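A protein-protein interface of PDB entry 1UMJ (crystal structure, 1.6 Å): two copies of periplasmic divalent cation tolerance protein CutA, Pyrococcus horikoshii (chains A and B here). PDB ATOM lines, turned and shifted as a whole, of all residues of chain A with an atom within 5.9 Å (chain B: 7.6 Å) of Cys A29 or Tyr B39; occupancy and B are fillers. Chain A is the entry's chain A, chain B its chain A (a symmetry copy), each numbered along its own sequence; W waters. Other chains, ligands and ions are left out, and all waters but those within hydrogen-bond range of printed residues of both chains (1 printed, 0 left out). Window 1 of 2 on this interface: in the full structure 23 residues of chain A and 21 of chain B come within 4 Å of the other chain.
O of Leu A22 is in hydrogen-bond range of NE1 of Trp B40, at 2.9 Å. N of Phe B38 is in hydrogen-bond range of O of Ala A30, 2.9 Å away.
O of Lys A56 is in hydrogen-bond range of N of Ala A28 (2.9 Å). O of Cys A29 lies within hydrogen-bond range of N of Lys A56. The side-chain sulfur of Cys A29 is in hydrogen-bond range of the side-chain hydroxyl of Tyr A92, 3.7 Å away. ND2 of Asn A31 sits close to NZ of Lys A56, 3.5 Å away. The backbone NH (N) of Ala B37 is in hydrogen-bond range of the backbone carbonyl oxygen (O) of Asp B48. O of Tyr B39 sits at hydrogen-bond distance from N of Glu B46 (2.6 Å).
Among the printed residues, merely in contact across the chains: Cys A29 with Phe B38 (3.2 Å), Ala A30 with Ala B37 (3.4 Å), Asn A31 with Arg B36 (3.5 Å), Tyr A92 with Ala B79 (3.6 Å), Cys A29 with Tyr B39 (3.6 Å), Ala A28 with Tyr B39 (3.6 Å), Leu A22 with Phe B38 (3.7 Å), Leu A22 with Ile B45 (3.7 Å), Trp A95 with Glu B42 (3.7 Å), Ala A30 with Arg B36 (3.7 Å), Asn A31 with Ala B37 (3.9 Å) and Trp A95 with Trp B40 (3.9 Å).
Cys A29 touches just these residues of chain B: Phe B38 and Tyr B39. Tyr B39 touches two residues of chain A. Of chain B, only Tyr B39 comes within 4 Å of Ala A28. Of the printed residues of chain A, Trp B40 touches Leu A22 and Trp A95. Of the printed residues of chain A, Ile B45 touches Leu A22. Of the printed residues of chain A, Ala B37 touches Ala A30 (3.4 Å) and Asn A31 (3.9 Å). Of the printed residues of chain A, Ala B79 touches Tyr A92. Printed residues of chain B within 4 Å of Asn A31: Arg B36 and Ala B37. Lys A56 touches none of the printed residues of chain B. Ile A27 touches none of the printed residues of chain B. The nearest printed residue of chain A that does not touch Phe B38 is Ala A28 (4.5 Å).
Of the 12 printed residues of chain A, 7 touch a printed residue of chain B. Hydrophobic or aromatic side chains of chain A that line the printed part of chain B: Leu A22, Tyr A92 and Trp A95. Of the 18 printed residues of chain B, 8 touch a printed residue of chain A. Among the printed residues, no Asp or Glu carboxylate lies within 4 Å of a Lys or Arg side-chain nitrogen of the other chain.
No position is printed for both chains.
Water W1 bridges the side-chain carboxylate of Glu B50 (2.7 Å) and the side-chain amide nitrogen of Asn A31 (3.3 Å).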
ATOM      1  N   LEU A  22      13.537  21.691 -12.372  1.00  0.00           N
ATOM      2  CA  LEU A  22      14.742  21.585 -13.205  1.00  0.00           C
ATOM      3  C   LEU A  22      14.324  21.365 -14.687  1.00  0.00           C
ATOM      4  O   LEU A  22      14.899  21.953 -15.596  1.00  0.00           O
ATOM      5  CB  LEU A  22      15.609  20.420 -12.741  1.00  0.00           C
ATOM      6  CG  LEU A  22      16.452  20.717 -11.482  1.00  0.00           C
ATOM      7  CD1 LEU A  22      16.884  19.462 -10.798  1.00  0.00           C
ATOM      8  CD2 LEU A  22      17.652  21.514 -11.888  1.00  0.00           C
ATOM      9  N   ILE A  27      15.186  26.526 -12.040  1.00  0.00           N
ATOM     10  CA  ILE A  27      16.303  26.500 -11.087  1.00  0.00           C
ATOM     11  C   ILE A  27      17.496  25.776 -11.734  1.00  0.00           C
ATOM     12  O   ILE A  27      17.326  24.976 -12.678  1.00  0.00           O
ATOM     13  CB  ILE A  27      15.928  25.803  -9.720  1.00  0.00           C
ATOM     14  CG1 ILE A  27      15.752  24.291  -9.910  1.00  0.00           C
ATOM     15  CG2 ILE A  27      14.716  26.455  -9.153  1.00  0.00           C
ATOM     16  CD1 ILE A  27      15.457  23.571  -8.565  1.00  0.00           C
ATOM     17  N   ALA A  28      18.708  26.096 -11.284  1.00  0.00           N
ATOM     18  CA  ALA A  28      19.936  25.459 -11.767  1.00  0.00           C
ATOM     19  C   ALA A  28      20.251  24.194 -10.950  1.00  0.00           C
ATOM     20  O   ALA A  28      20.880  23.249 -11.444  1.00  0.00           O
ATOM     21  CB  ALA A  28      21.124  26.443 -11.678  1.00  0.00           C
ATOM     22  N   CYS A  29      19.855  24.191  -9.682  1.00  0.00           N
ATOM     23  CA  CYS A  29      20.112  23.020  -8.849  1.00  0.00           C
ATOM     24  C   CYS A  29      19.337  23.111  -7.574  1.00  0.00           C
ATOM     25  O   CYS A  29      18.876  24.177  -7.199  1.00  0.00           O
ATOM     26  CB  CYS A  29      21.591  22.848  -8.567  1.00  0.00           C
ATOM     27  SG  CYS A  29      22.232  24.152  -7.642  1.00  0.00           S
ATOM     28  N   ALA A  30      19.152  21.946  -6.962  1.00  0.00           N
ATOM     29  CA  ALA A  30      18.427  21.856  -5.704  1.00  0.00           C
ATOM     30  C   ALA A  30      19.244  20.980  -4.778  1.00  0.00           C
ATOM     31  O   ALA A  30      19.802  19.992  -5.217  1.00  0.00           O
ATOM     32  CB  ALA A  30      17.062  21.225  -5.942  1.00  0.00           C
ATOM     33  N   ASN A  31      19.284  21.344  -3.481  1.00  0.00           N
ATOM     34  CA  ASN A  31      19.961  20.557  -2.459  1.00  0.00           C
ATOM     35  C   ASN A  31      18.842  20.192  -1.498  1.00  0.00           C
ATOM     36  O   ASN A  31      18.195  21.075  -0.918  1.00  0.00           O
ATOM     37  CB  ASN A  31      20.995  21.401  -1.709  1.00  0.00           C
ATOM     38  CG  ASN A  31      22.222  21.740  -2.556  1.00  0.00           C
ATOM     39  OD1 ASN A  31      23.057  22.549  -2.139  1.00  0.00           O
ATOM     40  ND2 ASN A  31      22.343  21.114  -3.748  1.00  0.00           N
ATOM     41  N   ILE A  54      16.914  23.630  -0.786  1.00  0.00           N
ATOM     42  CA  ILE A  54      17.662  24.858  -1.059  1.00  0.00           C
ATOM     43  C   ILE A  54      17.767  24.922  -2.586  1.00  0.00           C
ATOM     44  O   ILE A  54      18.462  24.086  -3.211  1.00  0.00           O
ATOM     45  CB  ILE A  54      19.076  24.771  -0.456  1.00  0.00           C
ATOM     46  CG1 ILE A  54      18.959  24.837   1.075  1.00  0.00           C
ATOM     47  CG2 ILE A  54      19.950  25.941  -0.997  1.00  0.00           C
ATOM     48  CD1 ILE A  54      20.245  24.883   1.768  1.00  0.00           C
ATOM     49  N   LEU A  55      17.115  25.906  -3.182  1.00  0.00           N
ATOM     50  CA  LEU A  55      17.083  26.046  -4.631  1.00  0.00           C
ATOM     51  C   LEU A  55      17.981  27.216  -5.044  1.00  0.00           C
ATOM     52  O   LEU A  55      17.968  28.250  -4.393  1.00  0.00           O
ATOM     53  CB  LEU A  55      15.647  26.282  -5.063  1.00  0.00           C
ATOM     54  CG  LEU A  55      14.613  25.340  -4.437  1.00  0.00           C
ATOM     55  CD1 LEU A  55      13.217  25.715  -4.923  1.00  0.00           C
ATOM     56  CD2 LEU A  55      14.995  23.820  -4.807  1.00  0.00           C
ATOM     57  N   LYS A  56      18.751  27.040  -6.120  1.00  0.00           N
ATOM     58  CA  LYS A  56      19.633  28.104  -6.608  1.00  0.00           C
ATOM     59  C   LYS A  56      19.191  28.512  -7.975  1.00  0.00           C
ATOM     60  O   LYS A  56      19.131  27.702  -8.876  1.00  0.00           O
ATOM     61  CB  LYS A  56      21.093  27.660  -6.675  1.00  0.00           C
ATOM     62  CG  LYS A  56      21.787  27.451  -5.321  1.00  0.00           C
ATOM     63  CD  LYS A  56      21.095  26.383  -4.500  1.00  0.00           C
ATOM     64  CE  LYS A  56      21.591  25.020  -4.879  1.00  0.00           C
ATOM     65  NZ  LYS A  56      20.624  24.012  -4.510  1.00  0.00           N
ATOM     66  N   THR A  57      18.895  29.790  -8.108  1.00  0.00           N
ATOM     67  CA  THR A  57      18.483  30.250  -9.423  1.00  0.00           C
ATOM     68  C   THR A  57      18.800  31.721  -9.636  1.00  0.00           C
ATOM     69  O   THR A  57      19.447  32.372  -8.804  1.00  0.00           O
ATOM     70  CB  THR A  57      16.990  29.961  -9.615  1.00  0.00           C
ATOM     71  OG1 THR A  57      16.651  30.082 -11.012  1.00  0.00           O
ATOM     72  CG2 THR A  57      16.155  30.864  -8.813  1.00  0.00           C
ATOM     73  N   TYR A  92      30.772  30.189 -11.553  1.00  0.00           N
ATOM     74  CA  TYR A  92      29.596  29.472 -11.096  1.00  0.00           C
ATOM     75  C   TYR A  92      28.339  30.236 -11.513  1.00  0.00           C
ATOM     76  O   TYR A  92      27.358  29.630 -11.961  1.00  0.00           O
ATOM     77  CB  TYR A  92      29.629  29.281  -9.560  1.00  0.00           C
ATOM     78  CG  TYR A  92      28.371  28.604  -9.071  1.00  0.00           C
ATOM     79  CD1 TYR A  92      28.242  27.226  -9.148  1.00  0.00           C
ATOM     80  CD2 TYR A  92      27.272  29.365  -8.616  1.00  0.00           C
ATOM     81  CE1 TYR A  92      27.054  26.610  -8.798  1.00  0.00           C
ATOM     82  CE2 TYR A  92      26.085  28.756  -8.263  1.00  0.00           C
ATOM     83  CZ  TYR A  92      25.982  27.374  -8.357  1.00  0.00           C
ATOM     84  OH  TYR A  92      24.798  26.773  -7.989  1.00  0.00           O
ATOM     85  N   TRP A  95      27.574  29.468 -15.146  1.00  0.00           N
ATOM     86  CA  TRP A  95      26.989  28.125 -15.261  1.00  0.00           C
ATOM     87  C   TRP A  95      25.495  28.182 -14.867  1.00  0.00           C
ATOM     88  O   TRP A  95      24.634  27.669 -15.556  1.00  0.00           O
ATOM     89  CB  TRP A  95      27.742  27.168 -14.342  1.00  0.00           C
ATOM     90  CG  TRP A  95      27.094  25.810 -14.226  1.00  0.00           C
ATOM     91  CD1 TRP A  95      27.263  24.744 -15.070  1.00  0.00           C
ATOM     92  CD2 TRP A  95      26.188  25.367 -13.194  1.00  0.00           C
ATOM     93  NE1 TRP A  95      26.524  23.667 -14.627  1.00  0.00           N
ATOM     94  CE2 TRP A  95      25.857  24.023 -13.476  1.00  0.00           C
ATOM     95  CE3 TRP A  95      25.625  25.978 -12.059  1.00  0.00           C
ATOM     96  CZ2 TRP A  95      24.985  23.274 -12.664  1.00  0.00           C
ATOM     97  CZ3 TRP A  95      24.757  25.238 -11.257  1.00  0.00           C
ATOM     98  CH2 TRP A  95      24.443  23.895 -11.566  1.00  0.00           C
ATOM     99  N   ARG B  36      21.212  15.728  -0.805  1.00  0.00           N
ATOM    100  CA  ARG B  36      21.066  15.086  -2.124  1.00  0.00           C
ATOM    101  C   ARG B  36      20.927  16.239  -3.067  1.00  0.00           C
ATOM    102  O   ARG B  36      20.055  17.109  -2.902  1.00  0.00           O
ATOM    103  CB  ARG B  36      19.831  14.170  -2.160  1.00  0.00           C
ATOM    104  CG  ARG B  36      20.061  12.927  -1.308  1.00  0.00           C
ATOM    105  CD  ARG B  36      18.903  11.899  -1.391  1.00  0.00           C
ATOM    106  NE  ARG B  36      19.257  10.627  -0.719  1.00  0.00           N
ATOM    107  CZ  ARG B  36      20.206   9.771  -1.132  1.00  0.00           C
ATOM    108  NH1 ARG B  36      20.937  10.016  -2.222  1.00  0.00           N
ATOM    109  NH2 ARG B  36      20.396   8.626  -0.469  1.00  0.00           N
ATOM    110  N   ALA B  37      21.800  16.233  -4.067  1.00  0.00           N
ATOM    111  CA  ALA B  37      21.826  17.299  -5.020  1.00  0.00           C
ATOM    112  C   ALA B  37      21.196  16.845  -6.335  1.00  0.00           C
ATOM    113  O   ALA B  37      21.387  15.687  -6.735  1.00  0.00           O
ATOM    114  CB  ALA B  37      23.329  17.695  -5.251  1.00  0.00           C
ATOM    115  N   PHE B  38      20.441  17.731  -6.953  1.00  0.00           N
ATOM    116  CA  PHE B  38      19.775  17.471  -8.241  1.00  0.00           C
ATOM    117  C   PHE B  38      20.151  18.624  -9.144  1.00  0.00           C
ATOM    118  O   PHE B  38      19.931  19.783  -8.813  1.00  0.00           O
ATOM    119  CB  PHE B  38      18.249  17.406  -8.105  1.00  0.00           C
ATOM    120  CG  PHE B  38      17.768  16.369  -7.140  1.00  0.00           C
ATOM    121  CD1 PHE B  38      17.939  16.561  -5.768  1.00  0.00           C
ATOM    122  CD2 PHE B  38      17.160  15.214  -7.591  1.00  0.00           C
ATOM    123  CE1 PHE B  38      17.510  15.621  -4.847  1.00  0.00           C
ATOM    124  CE2 PHE B  38      16.716  14.238  -6.667  1.00  0.00           C
ATOM    125  CZ  PHE B  38      16.897  14.447  -5.295  1.00  0.00           C
ATOM    126  N   TYR B  39      20.741  18.312 -10.298  1.00  0.00           N
ATOM    127  CA  TYR B  39      21.109  19.411 -11.186  1.00  0.00           C
ATOM    128  C   TYR B  39      21.318  18.828 -12.577  1.00  0.00           C
ATOM    129  O   TYR B  39      21.321  17.610 -12.749  1.00  0.00           O
ATOM    130  CB  TYR B  39      22.409  20.043 -10.700  1.00  0.00           C
ATOM    131  CG  TYR B  39      23.501  19.022 -10.471  1.00  0.00           C
ATOM    132  CD1 TYR B  39      23.514  18.229  -9.323  1.00  0.00           C
ATOM    133  CD2 TYR B  39      24.545  18.855 -11.394  1.00  0.00           C
ATOM    134  CE1 TYR B  39      24.528  17.297  -9.080  1.00  0.00           C
ATOM    135  CE2 TYR B  39      25.568  17.923 -11.160  1.00  0.00           C
ATOM    136  CZ  TYR B  39      25.561  17.155 -10.008  1.00  0.00           C
ATOM    137  OH  TYR B  39      26.578  16.260  -9.752  1.00  0.00           O
ATOM    138  N   TRP B  40      21.460  19.722 -13.556  1.00  0.00           N
ATOM    139  CA  TRP B  40      21.717  19.340 -14.938  1.00  0.00           C
ATOM    140  C   TRP B  40      23.219  19.216 -15.030  1.00  0.00           C
ATOM    141  O   TRP B  40      23.941  20.132 -14.658  1.00  0.00           O
ATOM    142  CB  TRP B  40      21.296  20.445 -15.928  1.00  0.00           C
ATOM    143  CG  TRP B  40      19.839  20.646 -16.121  1.00  0.00           C
ATOM    144  CD1 TRP B  40      19.037  21.570 -15.525  1.00  0.00           C
ATOM    145  CD2 TRP B  40      19.014  19.915 -17.025  1.00  0.00           C
ATOM    146  NE1 TRP B  40      17.746  21.460 -16.005  1.00  0.00           N
ATOM    147  CE2 TRP B  40      17.707  20.452 -16.932  1.00  0.00           C
ATOM    148  CE3 TRP B  40      19.256  18.855 -17.901  1.00  0.00           C
ATOM    149  CZ2 TRP B  40      16.637  19.958 -17.696  1.00  0.00           C
ATOM    150  CZ3 TRP B  40      18.202  18.358 -18.658  1.00  0.00           C
ATOM    151  CH2 TRP B  40      16.907  18.910 -18.554  1.00  0.00           C
ATOM    152  N   TRP B  41      23.689  18.076 -15.482  1.00  0.00           N
ATOM    153  CA  TRP B  41      25.117  17.905 -15.629  1.00  0.00           C
ATOM    154  C   TRP B  41      25.358  18.195 -17.100  1.00  0.00           C
ATOM    155  O   TRP B  41      25.966  17.413 -17.829  1.00  0.00           O
ATOM    156  CB  TRP B  41      25.533  16.488 -15.257  1.00  0.00           C
ATOM    157  CG  TRP B  41      27.009  16.314 -15.233  1.00  0.00           C
ATOM    158  CD1 TRP B  41      27.941  17.242 -14.863  1.00  0.00           C
ATOM    159  CD2 TRP B  41      27.724  15.119 -15.526  1.00  0.00           C
ATOM    160  NE1 TRP B  41      29.201  16.690 -14.903  1.00  0.00           N
ATOM    161  CE2 TRP B  41      29.096  15.385 -15.307  1.00  0.00           C
ATOM    162  CE3 TRP B  41      27.343  13.842 -15.951  1.00  0.00           C
ATOM    163  CZ2 TRP B  41      30.087  14.418 -15.498  1.00  0.00           C
ATOM    164  CZ3 TRP B  41      28.327  12.878 -16.142  1.00  0.00           C
ATOM    165  CH2 TRP B  41      29.682  13.171 -15.913  1.00  0.00           C
ATOM    166  N   GLU B  42      24.830  19.341 -17.532  1.00  0.00           N
ATOM    167  CA  GLU B  42      24.973  19.763 -18.912  1.00  0.00           C
ATOM    168  C   GLU B  42      24.419  18.626 -19.788  1.00  0.00           C
ATOM    169  O   GLU B  42      25.158  17.778 -20.304  1.00  0.00           O
ATOM    170  CB  GLU B  42      26.460  20.014 -19.194  1.00  0.00           C
ATOM    171  CG  GLU B  42      27.162  20.908 -18.148  1.00  0.00           C
ATOM    172  CD  GLU B  42      26.737  22.370 -18.226  1.00  0.00           C
ATOM    173  OE1 GLU B  42      25.527  22.642 -18.104  1.00  0.00           O
ATOM    174  OE2 GLU B  42      27.612  23.253 -18.402  1.00  0.00           O
ATOM    175  N   GLY B  43      23.106  18.590 -19.950  1.00  0.00           N
ATOM    176  CA  GLY B  43      22.552  17.527 -20.754  1.00  0.00           C
ATOM    177  C   GLY B  43      21.399  16.805 -20.108  1.00  0.00           C
ATOM    178  O   GLY B  43      20.305  16.804 -20.671  1.00  0.00           O
ATOM    179  N   LYS B  44      21.616  16.192 -18.945  1.00  0.00           N
ATOM    180  CA  LYS B  44      20.546  15.453 -18.268  1.00  0.00           C
ATOM    181  C   LYS B  44      20.482  15.701 -16.758  1.00  0.00           C
ATOM    182  O   LYS B  44      21.492  15.989 -16.135  1.00  0.00           O
ATOM    183  CB  LYS B  44      20.719  13.949 -18.478  1.00  0.00           C
ATOM    184  CG  LYS B  44      20.650  13.500 -19.927  1.00  0.00           C
ATOM    185  CD  LYS B  44      21.009  12.014 -20.096  1.00  0.00           C
ATOM    186  CE  LYS B  44      19.894  11.089 -19.648  1.00  0.00           C
ATOM    187  NZ  LYS B  44      20.247   9.646 -19.805  1.00  0.00           N
ATOM    188  N   ILE B  45      19.298  15.548 -16.177  1.00  0.00           N
ATOM    189  CA  ILE B  45      19.164  15.743 -14.731  1.00  0.00           C
ATOM    190  C   ILE B  45      19.923  14.652 -13.997  1.00  0.00           C
ATOM    191  O   ILE B  45      19.669  13.467 -14.211  1.00  0.00           O
ATOM    192  CB  ILE B  45      17.715  15.651 -14.266  1.00  0.00           C
ATOM    193  CG1 ILE B  45      16.843  16.689 -14.962  1.00  0.00           C
ATOM    194  CG2 ILE B  45      17.649  15.827 -12.752  1.00  0.00           C
ATOM    195  CD1 ILE B  45      17.332  18.044 -14.926  1.00  0.00           C
ATOM    196  N   GLU B  46      20.841  15.042 -13.112  1.00  0.00           N
ATOM    197  CA  GLU B  46      21.613  14.071 -12.351  1.00  0.00           C
ATOM    198  C   GLU B  46      21.293  14.219 -10.873  1.00  0.00           C
ATOM    199  O   GLU B  46      20.922  15.311 -10.419  1.00  0.00           O
ATOM    200  CB  GLU B  46      23.118  14.321 -12.522  1.00  0.00           C
ATOM    201  CG  GLU B  46      23.708  13.956 -13.874  1.00  0.00           C
ATOM    202  CD  GLU B  46      23.817  12.462 -14.065  1.00  0.00           C
ATOM    203  OE1 GLU B  46      22.779  11.779 -13.949  1.00  0.00           O
ATOM    204  OE2 GLU B  46      24.936  11.973 -14.341  1.00  0.00           O
ATOM    205  N   GLU B  47      21.407  13.114 -10.139  1.00  0.00           N
ATOM    206  CA  GLU B  47      21.211  13.125  -8.675  1.00  0.00           C
ATOM    207  C   GLU B  47      22.444  12.461  -8.018  1.00  0.00           C
ATOM    208  O   GLU B  47      22.995  11.486  -8.523  1.00  0.00           O
ATOM    209  CB  GLU B  47      19.927  12.350  -8.251  1.00  0.00           C
ATOM    210  CG  GLU B  47      18.716  12.393  -9.258  1.00  0.00           C
ATOM    211  CD  GLU B  47      17.338  11.888  -8.732  1.00  0.00           C
ATOM    212  OE1 GLU B  47      17.267  10.830  -8.069  1.00  0.00           O
ATOM    213  OE2 GLU B  47      16.302  12.561  -9.018  1.00  0.00           O
ATOM    214  N   ASP B  48      22.917  13.013  -6.905  1.00  0.00           N
ATOM    215  CA  ASP B  48      24.002  12.375  -6.167  1.00  0.00           C
ATOM    216  C   ASP B  48      24.179  13.034  -4.820  1.00  0.00           C
ATOM    217  O   ASP B  48      23.800  14.203  -4.620  1.00  0.00           O
ATOM    218  CB  ASP B  48      25.323  12.417  -6.936  1.00  0.00           C
ATOM    219  CG  ASP B  48      25.661  13.785  -7.422  1.00  0.00           C
ATOM    220  OD1 ASP B  48      26.145  13.902  -8.566  1.00  0.00           O
ATOM    221  OD2 ASP B  48      25.455  14.752  -6.677  1.00  0.00           O
ATOM    222  N   LYS B  49      24.766  12.284  -3.908  1.00  0.00           N
ATOM    223  CA  LYS B  49      24.982  12.788  -2.578  1.00  0.00           C
ATOM    224  C   LYS B  49      26.221  13.650  -2.549  1.00  0.00           C
ATOM    225  O   LYS B  49      27.249  13.343  -3.169  1.00  0.00           O
ATOM    226  CB  LYS B  49      25.072  11.628  -1.597  1.00  0.00           C
ATOM    227  CG  LYS B  49      25.518  12.015  -0.221  1.00  0.00           C
ATOM    228  CD  LYS B  49      25.796  10.771   0.640  1.00  0.00           C
ATOM    229  CE  LYS B  49      24.513   9.990   0.917  1.00  0.00           C
ATOM    230  NZ  LYS B  49      23.425  10.887   1.416  1.00  0.00           N
ATOM    231  N   GLU B  50      26.093  14.795  -1.885  1.00  0.00           N
ATOM    232  CA  GLU B  50      27.206  15.700  -1.741  1.00  0.00           C
ATOM    233  C   GLU B  50      27.303  16.167  -0.261  1.00  0.00           C
ATOM    234  O   GLU B  50      26.458  15.868   0.588  1.00  0.00           O
ATOM    235  CB  GLU B  50      26.991  16.952  -2.557  1.00  0.00           C
ATOM    236  CG  GLU B  50      26.677  16.819  -3.996  1.00  0.00           C
ATOM    237  CD  GLU B  50      26.682  18.207  -4.647  1.00  0.00           C
ATOM    238  OE1 GLU B  50      26.029  19.192  -4.141  1.00  0.00           O
ATOM    239  OE2 GLU B  50      27.358  18.312  -5.653  1.00  0.00           O
ATOM    240  N   TYR B  75      36.173  20.401  -7.367  1.00  0.00           N
ATOM    241  CA  TYR B  75      35.440  20.813  -8.568  1.00  0.00           C
ATOM    242  C   TYR B  75      36.159  21.951  -9.307  1.00  0.00           C
ATOM    243  O   TYR B  75      36.710  22.856  -8.684  1.00  0.00           O
ATOM    244  CB  TYR B  75      34.005  21.301  -8.255  1.00  0.00           C
ATOM    245  CG  TYR B  75      33.031  20.292  -7.636  1.00  0.00           C
ATOM    246  CD1 TYR B  75      33.108  18.927  -7.937  1.00  0.00           C
ATOM    247  CD2 TYR B  75      31.974  20.712  -6.833  1.00  0.00           C
ATOM    248  CE1 TYR B  75      32.150  18.019  -7.456  1.00  0.00           C
ATOM    249  CE2 TYR B  75      31.002  19.806  -6.346  1.00  0.00           C
ATOM    250  CZ  TYR B  75      31.100  18.457  -6.668  1.00  0.00           C
ATOM    251  OH  TYR B  75      30.115  17.555  -6.268  1.00  0.00           O
ATOM    252  N   ALA B  79      30.758  25.982  -6.309  1.00  0.00           N
ATOM    253  CA  ALA B  79      29.867  27.066  -5.930  1.00  0.00           C
ATOM    254  C   ALA B  79      30.532  27.761  -4.746  1.00  0.00           C
ATOM    255  O   ALA B  79      30.886  27.092  -3.786  1.00  0.00           O
ATOM    256  CB  ALA B  79      28.528  26.463  -5.490  1.00  0.00           C
ATOM    257  N   ILE B  81      29.361  30.753  -2.522  1.00  0.00           N
ATOM    258  CA  ILE B  81      28.288  31.708  -2.314  1.00  0.00           C
ATOM    259  C   ILE B  81      28.388  32.502  -1.010  1.00  0.00           C
ATOM    260  O   ILE B  81      28.584  31.936   0.081  1.00  0.00           O
ATOM    261  CB  ILE B  81      26.958  30.918  -2.398  1.00  0.00           C
ATOM    262  CG1 ILE B  81      26.778  30.425  -3.840  1.00  0.00           C
ATOM    263  CG2 ILE B  81      25.796  31.764  -1.995  1.00  0.00           C
ATOM    264  CD1 ILE B  81      25.746  29.320  -3.954  1.00  0.00           C
HETATM  265  O   HOH W   1      25.165  21.383  -5.404  1.00  0.00           O
